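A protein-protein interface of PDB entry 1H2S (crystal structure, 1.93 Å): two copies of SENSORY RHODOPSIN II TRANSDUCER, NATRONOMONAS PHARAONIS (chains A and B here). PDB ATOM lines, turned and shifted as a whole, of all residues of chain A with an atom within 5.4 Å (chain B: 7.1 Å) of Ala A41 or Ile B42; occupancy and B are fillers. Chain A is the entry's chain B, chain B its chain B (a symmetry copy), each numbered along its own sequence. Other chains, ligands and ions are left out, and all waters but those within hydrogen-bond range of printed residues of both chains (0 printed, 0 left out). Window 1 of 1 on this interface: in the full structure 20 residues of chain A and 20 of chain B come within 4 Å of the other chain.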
ATOM      1  N   PHE A  14       9.199  21.738  21.289  1.00  0.00           N
ATOM      2  CA  PHE A  14       8.118  21.847  20.314  1.00  0.00           C
ATOM      3  C   PHE A  14       8.513  21.131  19.033  1.00  0.00           C
ATOM      4  O   PHE A  14       7.702  20.436  18.409  1.00  0.00           O
ATOM      5  CB  PHE A  14       7.835  23.312  20.013  1.00  0.00           C
ATOM      6  CG  PHE A  14       6.595  23.531  19.203  1.00  0.00           C
ATOM      7  CD1 PHE A  14       5.346  23.573  19.822  1.00  0.00           C
ATOM      8  CD2 PHE A  14       6.665  23.666  17.827  1.00  0.00           C
ATOM      9  CE1 PHE A  14       4.186  23.751  19.064  1.00  0.00           C
ATOM     10  CE2 PHE A  14       5.514  23.843  17.062  1.00  0.00           C
ATOM     11  CZ  PHE A  14       4.273  23.883  17.686  1.00  0.00           C
ATOM     12  N   GLY A  15       9.772  21.317  18.638  1.00  0.00           N
ATOM     13  CA  GLY A  15      10.273  20.686  17.429  1.00  0.00           C
ATOM     14  C   GLY A  15      10.188  19.181  17.536  1.00  0.00           C
ATOM     15  O   GLY A  15       9.793  18.503  16.586  1.00  0.00           O
ATOM     16  N   ALA A  18       6.636  18.165  17.139  1.00  0.00           N
ATOM     17  CA  ALA A  18       6.295  18.332  15.729  1.00  0.00           C
ATOM     18  C   ALA A  18       6.923  17.199  14.921  1.00  0.00           C
ATOM     19  O   ALA A  18       6.267  16.591  14.075  1.00  0.00           O
ATOM     20  CB  ALA A  18       6.806  19.670  15.223  1.00  0.00           C
ATOM     21  N   TYR A  19       8.200  16.930  15.174  1.00  0.00           N
ATOM     22  CA  TYR A  19       8.909  15.850  14.489  1.00  0.00           C
ATOM     23  C   TYR A  19       8.165  14.523  14.699  1.00  0.00           C
ATOM     24  O   TYR A  19       8.011  13.721  13.770  1.00  0.00           O
ATOM     25  CB  TYR A  19      10.330  15.726  15.046  1.00  0.00           C
ATOM     26  CG  TYR A  19      11.115  14.567  14.472  1.00  0.00           C
ATOM     27  CD1 TYR A  19      11.430  14.519  13.118  1.00  0.00           C
ATOM     28  CD2 TYR A  19      11.534  13.512  15.282  1.00  0.00           C
ATOM     29  CE1 TYR A  19      12.148  13.447  12.575  1.00  0.00           C
ATOM     30  CE2 TYR A  19      12.252  12.433  14.754  1.00  0.00           C
ATOM     31  CZ  TYR A  19      12.555  12.410  13.400  1.00  0.00           C
ATOM     32  OH  TYR A  19      13.273  11.350  12.874  1.00  0.00           O
ATOM     33  N   VAL A  22       5.305  14.242  12.340  1.00  0.00           N
ATOM     34  CA  VAL A  22       5.744  14.017  10.968  1.00  0.00           C
ATOM     35  C   VAL A  22       6.163  12.563  10.768  1.00  0.00           C
ATOM     36  O   VAL A  22       5.812  11.951   9.763  1.00  0.00           O
ATOM     37  CB  VAL A  22       6.942  14.932  10.610  1.00  0.00           C
ATOM     38  CG1 VAL A  22       7.542  14.521   9.252  1.00  0.00           C
ATOM     39  CG2 VAL A  22       6.482  16.388  10.578  1.00  0.00           C
ATOM     40  N   GLU A  36       0.550  17.517   5.744  1.00  0.00           N
ATOM     41  CA  GLU A  36      -0.309  18.185   6.724  1.00  0.00           C
ATOM     42  C   GLU A  36       0.433  18.346   8.043  1.00  0.00           C
ATOM     43  O   GLU A  36       0.390  19.413   8.662  1.00  0.00           O
ATOM     44  CB  GLU A  36      -1.586  17.368   6.939  1.00  0.00           C
ATOM     45  CG  GLU A  36      -2.434  17.222   5.691  1.00  0.00           C
ATOM     46  CD  GLU A  36      -3.620  16.296   5.904  1.00  0.00           C
ATOM     47  OE1 GLU A  36      -4.340  16.032   4.920  1.00  0.00           O
ATOM     48  OE2 GLU A  36      -3.828  15.837   7.051  1.00  0.00           O
ATOM     49  N   ALA A  37       1.114  17.283   8.470  1.00  0.00           N
ATOM     50  CA  ALA A  37       1.890  17.341   9.707  1.00  0.00           C
ATOM     51  C   ALA A  37       3.052  18.335   9.584  1.00  0.00           C
ATOM     52  O   ALA A  37       3.399  19.007  10.547  1.00  0.00           O
ATOM     53  CB  ALA A  37       2.444  15.953  10.059  1.00  0.00           C
ATOM     54  N   ALA A  38       3.649  18.419   8.397  1.00  0.00           N
ATOM     55  CA  ALA A  38       4.786  19.308   8.164  1.00  0.00           C
ATOM     56  C   ALA A  38       4.367  20.777   8.155  1.00  0.00           C
ATOM     57  O   ALA A  38       5.032  21.630   8.743  1.00  0.00           O
ATOM     58  CB  ALA A  38       5.461  18.947   6.847  1.00  0.00           C
ATOM     59  N   VAL A  39       3.263  21.071   7.477  1.00  0.00           N
ATOM     60  CA  VAL A  39       2.762  22.435   7.425  1.00  0.00           C
ATOM     61  C   VAL A  39       2.401  22.906   8.839  1.00  0.00           C
ATOM     62  O   VAL A  39       2.646  24.056   9.209  1.00  0.00           O
ATOM     63  CB  VAL A  39       1.517  22.538   6.524  1.00  0.00           C
ATOM     64  CG1 VAL A  39       0.977  23.970   6.526  1.00  0.00           C
ATOM     65  CG2 VAL A  39       1.886  22.131   5.105  1.00  0.00           C
ATOM     66  N   SER A  40       1.830  21.993   9.621  1.00  0.00           N
ATOM     67  CA  SER A  40       1.437  22.293  10.989  1.00  0.00           C
ATOM     68  C   SER A  40       2.672  22.625  11.811  1.00  0.00           C
ATOM     69  O   SER A  40       2.674  23.571  12.603  1.00  0.00           O
ATOM     70  CB  SER A  40       0.711  21.080  11.588  1.00  0.00           C
ATOM     71  OG  SER A  40       0.492  21.246  12.980  1.00  0.00           O
ATOM     72  N   ALA A  41       3.736  21.852  11.598  1.00  0.00           N
ATOM     73  CA  ALA A  41       4.987  22.065  12.333  1.00  0.00           C
ATOM     74  C   ALA A  41       5.624  23.416  12.000  1.00  0.00           C
ATOM     75  O   ALA A  41       6.071  24.135  12.894  1.00  0.00           O
ATOM     76  CB  ALA A  41       5.990  20.890  12.030  1.00  0.00           C
ATOM     77  N   ILE A  42       5.653  23.760  10.717  1.00  0.00           N
ATOM     78  CA  ILE A  42       6.249  25.014  10.290  1.00  0.00           C
ATOM     79  C   ILE A  42       5.490  26.201  10.847  1.00  0.00           C
ATOM     80  O   ILE A  42       6.081  27.110  11.439  1.00  0.00           O
ATOM     81  CB  ILE A  42       6.294  25.098   8.741  1.00  0.00           C
ATOM     82  CG1 ILE A  42       7.231  24.007   8.200  1.00  0.00           C
ATOM     83  CG2 ILE A  42       6.754  26.490   8.302  1.00  0.00           C
ATOM     84  CD1 ILE A  42       7.226  23.883   6.677  1.00  0.00           C
ATOM     85  N   LEU A  43       4.170  26.181  10.681  1.00  0.00           N
ATOM     86  CA  LEU A  43       3.323  27.261  11.182  1.00  0.00           C
ATOM     87  C   LEU A  43       3.382  27.315  12.700  1.00  0.00           C
ATOM     88  O   LEU A  43       3.405  28.390  13.287  1.00  0.00           O
ATOM     89  CB  LEU A  43       1.876  27.048  10.721  1.00  0.00           C
ATOM     90  CG  LEU A  43       1.585  27.323   9.242  1.00  0.00           C
ATOM     91  CD1 LEU A  43       0.163  26.872   8.896  1.00  0.00           C
ATOM     92  CD2 LEU A  43       1.767  28.815   8.962  1.00  0.00           C
ATOM     93  N   GLY A  44       3.410  26.147  13.334  1.00  0.00           N
ATOM     94  CA  GLY A  44       3.469  26.111  14.781  1.00  0.00           C
ATOM     95  C   GLY A  44       4.755  26.735  15.300  1.00  0.00           C
ATOM     96  O   GLY A  44       4.738  27.451  16.303  1.00  0.00           O
ATOM     97  N   LEU A  45       5.879  26.456  14.633  1.00  0.00           N
ATOM     98  CA  LEU A  45       7.156  27.017  15.049  1.00  0.00           C
ATOM     99  C   LEU A  45       7.185  28.535  14.855  1.00  0.00           C
ATOM    100  O   LEU A  45       7.750  29.264  15.672  1.00  0.00           O
ATOM    101  CB  LEU A  45       8.310  26.357  14.272  1.00  0.00           C
ATOM    102  CG  LEU A  45       8.704  24.961  14.747  1.00  0.00           C
ATOM    103  CD1 LEU A  45       9.687  24.334  13.772  1.00  0.00           C
ATOM    104  CD2 LEU A  45       9.333  25.047  16.132  1.00  0.00           C
ATOM    105  N   ILE A  46       6.575  29.014  13.778  1.00  0.00           N
ATOM    106  CA  ILE A  46       6.511  30.446  13.534  1.00  0.00           C
ATOM    107  C   ILE A  46       5.689  31.111  14.655  1.00  0.00           C
ATOM    108  O   ILE A  46       6.056  32.168  15.175  1.00  0.00           O
ATOM    109  CB  ILE A  46       5.835  30.724  12.185  1.00  0.00           C
ATOM    110  CG1 ILE A  46       6.704  30.175  11.049  1.00  0.00           C
ATOM    111  CG2 ILE A  46       5.588  32.207  12.015  1.00  0.00           C
ATOM    112  CD1 ILE A  46       6.043  30.276   9.675  1.00  0.00           C
ATOM    113  N   PHE B  14      11.836  32.224   5.876  1.00  0.00           N
ATOM    114  CA  PHE B  14      12.436  30.896   5.939  1.00  0.00           C
ATOM    115  C   PHE B  14      11.344  29.840   5.896  1.00  0.00           C
ATOM    116  O   PHE B  14      11.475  28.807   5.227  1.00  0.00           O
ATOM    117  CB  PHE B  14      13.237  30.747   7.224  1.00  0.00           C
ATOM    118  CG  PHE B  14      14.076  29.507   7.271  1.00  0.00           C
ATOM    119  CD1 PHE B  14      15.330  29.480   6.663  1.00  0.00           C
ATOM    120  CD2 PHE B  14      13.608  28.361   7.891  1.00  0.00           C
ATOM    121  CE1 PHE B  14      16.102  28.316   6.683  1.00  0.00           C
ATOM    122  CE2 PHE B  14      14.369  27.194   7.916  1.00  0.00           C
ATOM    123  CZ  PHE B  14      15.618  27.175   7.308  1.00  0.00           C
ATOM    124  N   ALA B  18      10.868  26.830   3.322  1.00  0.00           N
ATOM    125  CA  ALA B  18      10.739  25.472   3.840  1.00  0.00           C
ATOM    126  C   ALA B  18       9.426  24.866   3.348  1.00  0.00           C
ATOM    127  O   ALA B  18       9.394  23.725   2.886  1.00  0.00           O
ATOM    128  CB  ALA B  18      10.762  25.488   5.359  1.00  0.00           C
ATOM    129  N   GLN B  35       8.873  13.621   4.275  1.00  0.00           N
ATOM    130  CA  GLN B  35       9.446  13.555   5.612  1.00  0.00           C
ATOM    131  C   GLN B  35      10.838  14.211   5.665  1.00  0.00           C
ATOM    132  O   GLN B  35      11.170  14.897   6.627  1.00  0.00           O
ATOM    133  CB  GLN B  35       9.542  12.095   6.063  1.00  0.00           C
ATOM    134  CG  GLN B  35      10.311  11.899   7.354  1.00  0.00           C
ATOM    135  CD  GLN B  35      10.369  10.449   7.782  1.00  0.00           C
ATOM    136  OE1 GLN B  35      10.627   9.560   6.969  1.00  0.00           O
ATOM    137  NE2 GLN B  35      10.137  10.200   9.065  1.00  0.00           N
ATOM    138  N   ALA B  37      12.007  16.583   3.669  1.00  0.00           N
ATOM    139  CA  ALA B  37      11.823  18.029   3.556  1.00  0.00           C
ATOM    140  C   ALA B  37      11.286  18.620   4.865  1.00  0.00           C
ATOM    141  O   ALA B  37      11.641  19.733   5.236  1.00  0.00           O
ATOM    142  CB  ALA B  37      10.852  18.359   2.413  1.00  0.00           C
ATOM    143  N   ALA B  38      10.427  17.874   5.557  1.00  0.00           N
ATOM    144  CA  ALA B  38       9.824  18.341   6.804  1.00  0.00           C
ATOM    145  C   ALA B  38      10.840  18.385   7.945  1.00  0.00           C
ATOM    146  O   ALA B  38      10.889  19.346   8.712  1.00  0.00           O
ATOM    147  CB  ALA B  38       8.653  17.442   7.178  1.00  0.00           C
ATOM    148  N   VAL B  39      11.645  17.336   8.057  1.00  0.00           N
ATOM    149  CA  VAL B  39      12.665  17.287   9.093  1.00  0.00           C
ATOM    150  C   VAL B  39      13.663  18.434   8.888  1.00  0.00           C
ATOM    151  O   VAL B  39      14.118  19.061   9.847  1.00  0.00           O
ATOM    152  CB  VAL B  39      13.423  15.947   9.069  1.00  0.00           C
ATOM    153  CG1 VAL B  39      14.524  15.939  10.132  1.00  0.00           C
ATOM    154  CG2 VAL B  39      12.445  14.811   9.334  1.00  0.00           C
ATOM    155  N   SER B  40      13.980  18.702   7.624  1.00  0.00           N
ATOM    156  CA  SER B  40      14.910  19.764   7.275  1.00  0.00           C
ATOM    157  C   SER B  40      14.333  21.104   7.703  1.00  0.00           C
ATOM    158  O   SER B  40      15.038  21.955   8.253  1.00  0.00           O
ATOM    159  CB  SER B  40      15.153  19.751   5.759  1.00  0.00           C
ATOM    160  OG  SER B  40      15.887  20.892   5.345  1.00  0.00           O
ATOM    161  N   ALA B  41      13.033  21.278   7.468  1.00  0.00           N
ATOM    162  CA  ALA B  41      12.359  22.530   7.828  1.00  0.00           C
ATOM    163  C   ALA B  41      12.343  22.758   9.342  1.00  0.00           C
ATOM    164  O   ALA B  41      12.615  23.863   9.812  1.00  0.00           O
ATOM    165  CB  ALA B  41      10.893  22.530   7.253  1.00  0.00           C
ATOM    166  N   ILE B  42      12.037  21.709  10.097  1.00  0.00           N
ATOM    167  CA  ILE B  42      11.978  21.819  11.545  1.00  0.00           C
ATOM    168  C   ILE B  42      13.337  22.155  12.126  1.00  0.00           C
ATOM    169  O   ILE B  42      13.474  23.094  12.916  1.00  0.00           O
ATOM    170  CB  ILE B  42      11.448  20.503  12.173  1.00  0.00           C
ATOM    171  CG1 ILE B  42       9.993  20.280  11.730  1.00  0.00           C
ATOM    172  CG2 ILE B  42      11.560  20.563  13.697  1.00  0.00           C
ATOM    173  CD1 ILE B  42       9.417  18.928  12.150  1.00  0.00           C
ATOM    174  N   LEU B  43      14.352  21.400  11.713  1.00  0.00           N
ATOM    175  CA  LEU B  43      15.714  21.628  12.190  1.00  0.00           C
ATOM    176  C   LEU B  43      16.211  22.989  11.729  1.00  0.00           C
ATOM    177  O   LEU B  43      16.888  23.690  12.471  1.00  0.00           O
ATOM    178  CB  LEU B  43      16.643  20.525  11.668  1.00  0.00           C
ATOM    179  CG  LEU B  43      16.499  19.147  12.321  1.00  0.00           C
ATOM    180  CD1 LEU B  43      17.338  18.117  11.560  1.00  0.00           C
ATOM    181  CD2 LEU B  43      16.939  19.236  13.783  1.00  0.00           C
ATOM    182  N   GLY B  44      15.870  23.359  10.499  1.00  0.00           N
ATOM    183  CA  GLY B  44      16.302  24.643   9.986  1.00  0.00           C
ATOM    184  C   GLY B  44      15.714  25.791  10.792  1.00  0.00           C
ATOM    185  O   GLY B  44      16.401  26.777  11.061  1.00  0.00           O
ATOM    186  N   LEU B  45      14.436  25.679  11.166  1.00  0.00           N
ATOM    187  CA  LEU B  45      13.791  26.722  11.949  1.00  0.00           C
ATOM    188  C   LEU B  45      14.398  26.819  13.351  1.00  0.00           C
ATOM    189  O   LEU B  45      14.551  27.913  13.898  1.00  0.00           O
ATOM    190  CB  LEU B  45      12.275  26.464  12.040  1.00  0.00           C
ATOM    191  CG  LEU B  45      11.474  26.827  10.793  1.00  0.00           C
ATOM    192  CD1 LEU B  45      10.046  26.323  10.923  1.00  0.00           C
ATOM    193  CD2 LEU B  45      11.474  28.338  10.602  1.00  0.00           C
ATOM    194  N   ILE B  46      14.747  25.679  13.934  1.00  0.00           N
ATOM    195  CA  ILE B  46      15.374  25.676  15.246  1.00  0.00           C
ATOM    196  C   ILE B  46      16.738  26.386  15.153  1.00  0.00           C
ATOM    197  O   ILE B  46      17.102  27.186  16.021  1.00  0.00           O
ATOM    198  CB  ILE B  46      15.592  24.234  15.725  1.00  0.00           C
ATOM    199  CG1 ILE B  46      14.238  23.551  15.940  1.00  0.00           C
ATOM    200  CG2 ILE B  46      16.418  24.220  16.993  1.00  0.00           C
ATOM    201  CD1 ILE B  46      14.353  22.065  16.278  1.00  0.00           C
ATOM    202  N   ILE B  47      17.492  26.089  14.094  1.00  0.00           N
ATOM    203  CA  ILE B  47      18.810  26.725  13.898  1.00  0.00           C
ATOM    204  C   ILE B  47      18.628  28.232  13.663  1.00  0.00           C
ATOM    205  O   ILE B  47      19.373  29.055  14.196  1.00  0.00           O
ATOM    206  CB  ILE B  47      19.545  26.095  12.695  1.00  0.00           C
ATOM    207  CG1 ILE B  47      19.936  24.649  13.026  1.00  0.00           C
ATOM    208  CG2 ILE B  47      20.795  26.884  12.371  1.00  0.00           C
ATOM    209  CD1 ILE B  47      20.509  23.892  11.838  1.00  0.00           C
ATOM    210  N   LEU B  48      17.638  28.586  12.851  1.00  0.00           N
ATOM    211  CA  LEU B  48      17.355  29.986  12.580  1.00  0.00           C
ATOM    212  C   LEU B  48      17.118  30.731  13.909  1.00  0.00           C
ATOM    213  O   LEU B  48      17.570  31.870  14.086  1.00  0.00           O
ATOM    214  CB  LEU B  48      16.123  30.104  11.691  1.00  0.00           C
ATOM    215  CG  LEU B  48      15.809  31.508  11.182  1.00  0.00           C
ATOM    216  CD1 LEU B  48      16.944  31.984  10.284  1.00  0.00           C
ATOM    217  CD2 LEU B  48      14.493  31.502  10.417  1.00  0.00           C
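Of the 15 printed residues of chain B, 5 touch a printed residue of chain A.
Hydrophobic or aromatic side chains of chain B that line the printed part of chain A: Ala B38, Val B39, Ala B41, Ile B42 and Leu B45.
Along chain B the printed residues that touch a printed residue of chain A span positions 38 to 45.
Printed residues of chain A that touch a printed residue of chain B: Gly A15, Tyr A19, Val A22, Ala A38, Ala A41, Ile A42 and Leu A45.
Hydrophobic or aromatic side chains of chain A within 4 Å of the printed part of chain B: Tyr A19, Val A22, Ala A38, Ala A41, Ile A42 and Leu A45.
Among the printed residues, 8 pairs touch across the chains.
Among the printed residues, no Asp or Glu carboxylate lies within 4 Å of a Lys or Arg side-chain nitrogen of the other chain.
Ala A38 touches its own counterpart, Ala B38.
Ala A41 touches Ile B42, and with the chains exchanged Ile A42 touches Ala B41.
Leu B45 touches its own counterpart, Leu A45.
Positions printed for both chains: 14, 18, 37, 38, 39, 40, 41, 42, 43, 44, 45 and 46.
Of the 8 pairs that touch across the chains among the printed residues, 4 have their exchanged pair printed and touching as well.
Among the printed residues, pairs that only touch across the chains: Gly A15 with Ile B42 (3.9 Å), Tyr A19 with Val B39 (3.5 Å), Tyr A19 with Ile B42 (3.8 Å), Val A22 with Ala B38 (3.8 Å), Ala A38 with Ala B38 (3.5 Å), Ala A41 with Ile B42 (3.95 Å), Ile A42 with Ala B41 (3.95 Å) and Leu A45 with Leu B45 (3.5 Å).
Printed residues of chain B within 4 Å of Tyr A19: Val B39 (3.5 Å) and Ile B42 (3.8 Å).
Of the printed residues of chain B, Ala A38 touches Ala B38.
Of chain B, only Ile B42 (3.95 Å) comes within 4 Å of Ala A41.
Printed residues of chain B within 4 Å of Ile A42: Ala B41 (3.95 Å).
Printed residues of chain B within 4 Å of Leu A45: Leu B45 (3.5 Å).
Ser B40 touches none of the printed residues of chain A.
Printed residues of chain A within 4 Å of Ala B41: Ile A42.
Of the printed residues of chain A, Ile B42 touches Gly A15, Tyr A19 and Ala A41.
The nearest residue of chain A that does not touch Ile B42 is Leu A45 (4.1 Å).
The nearest printed residue of chain A that does not touch Leu B45 is Ile A42 (4.1 Å).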
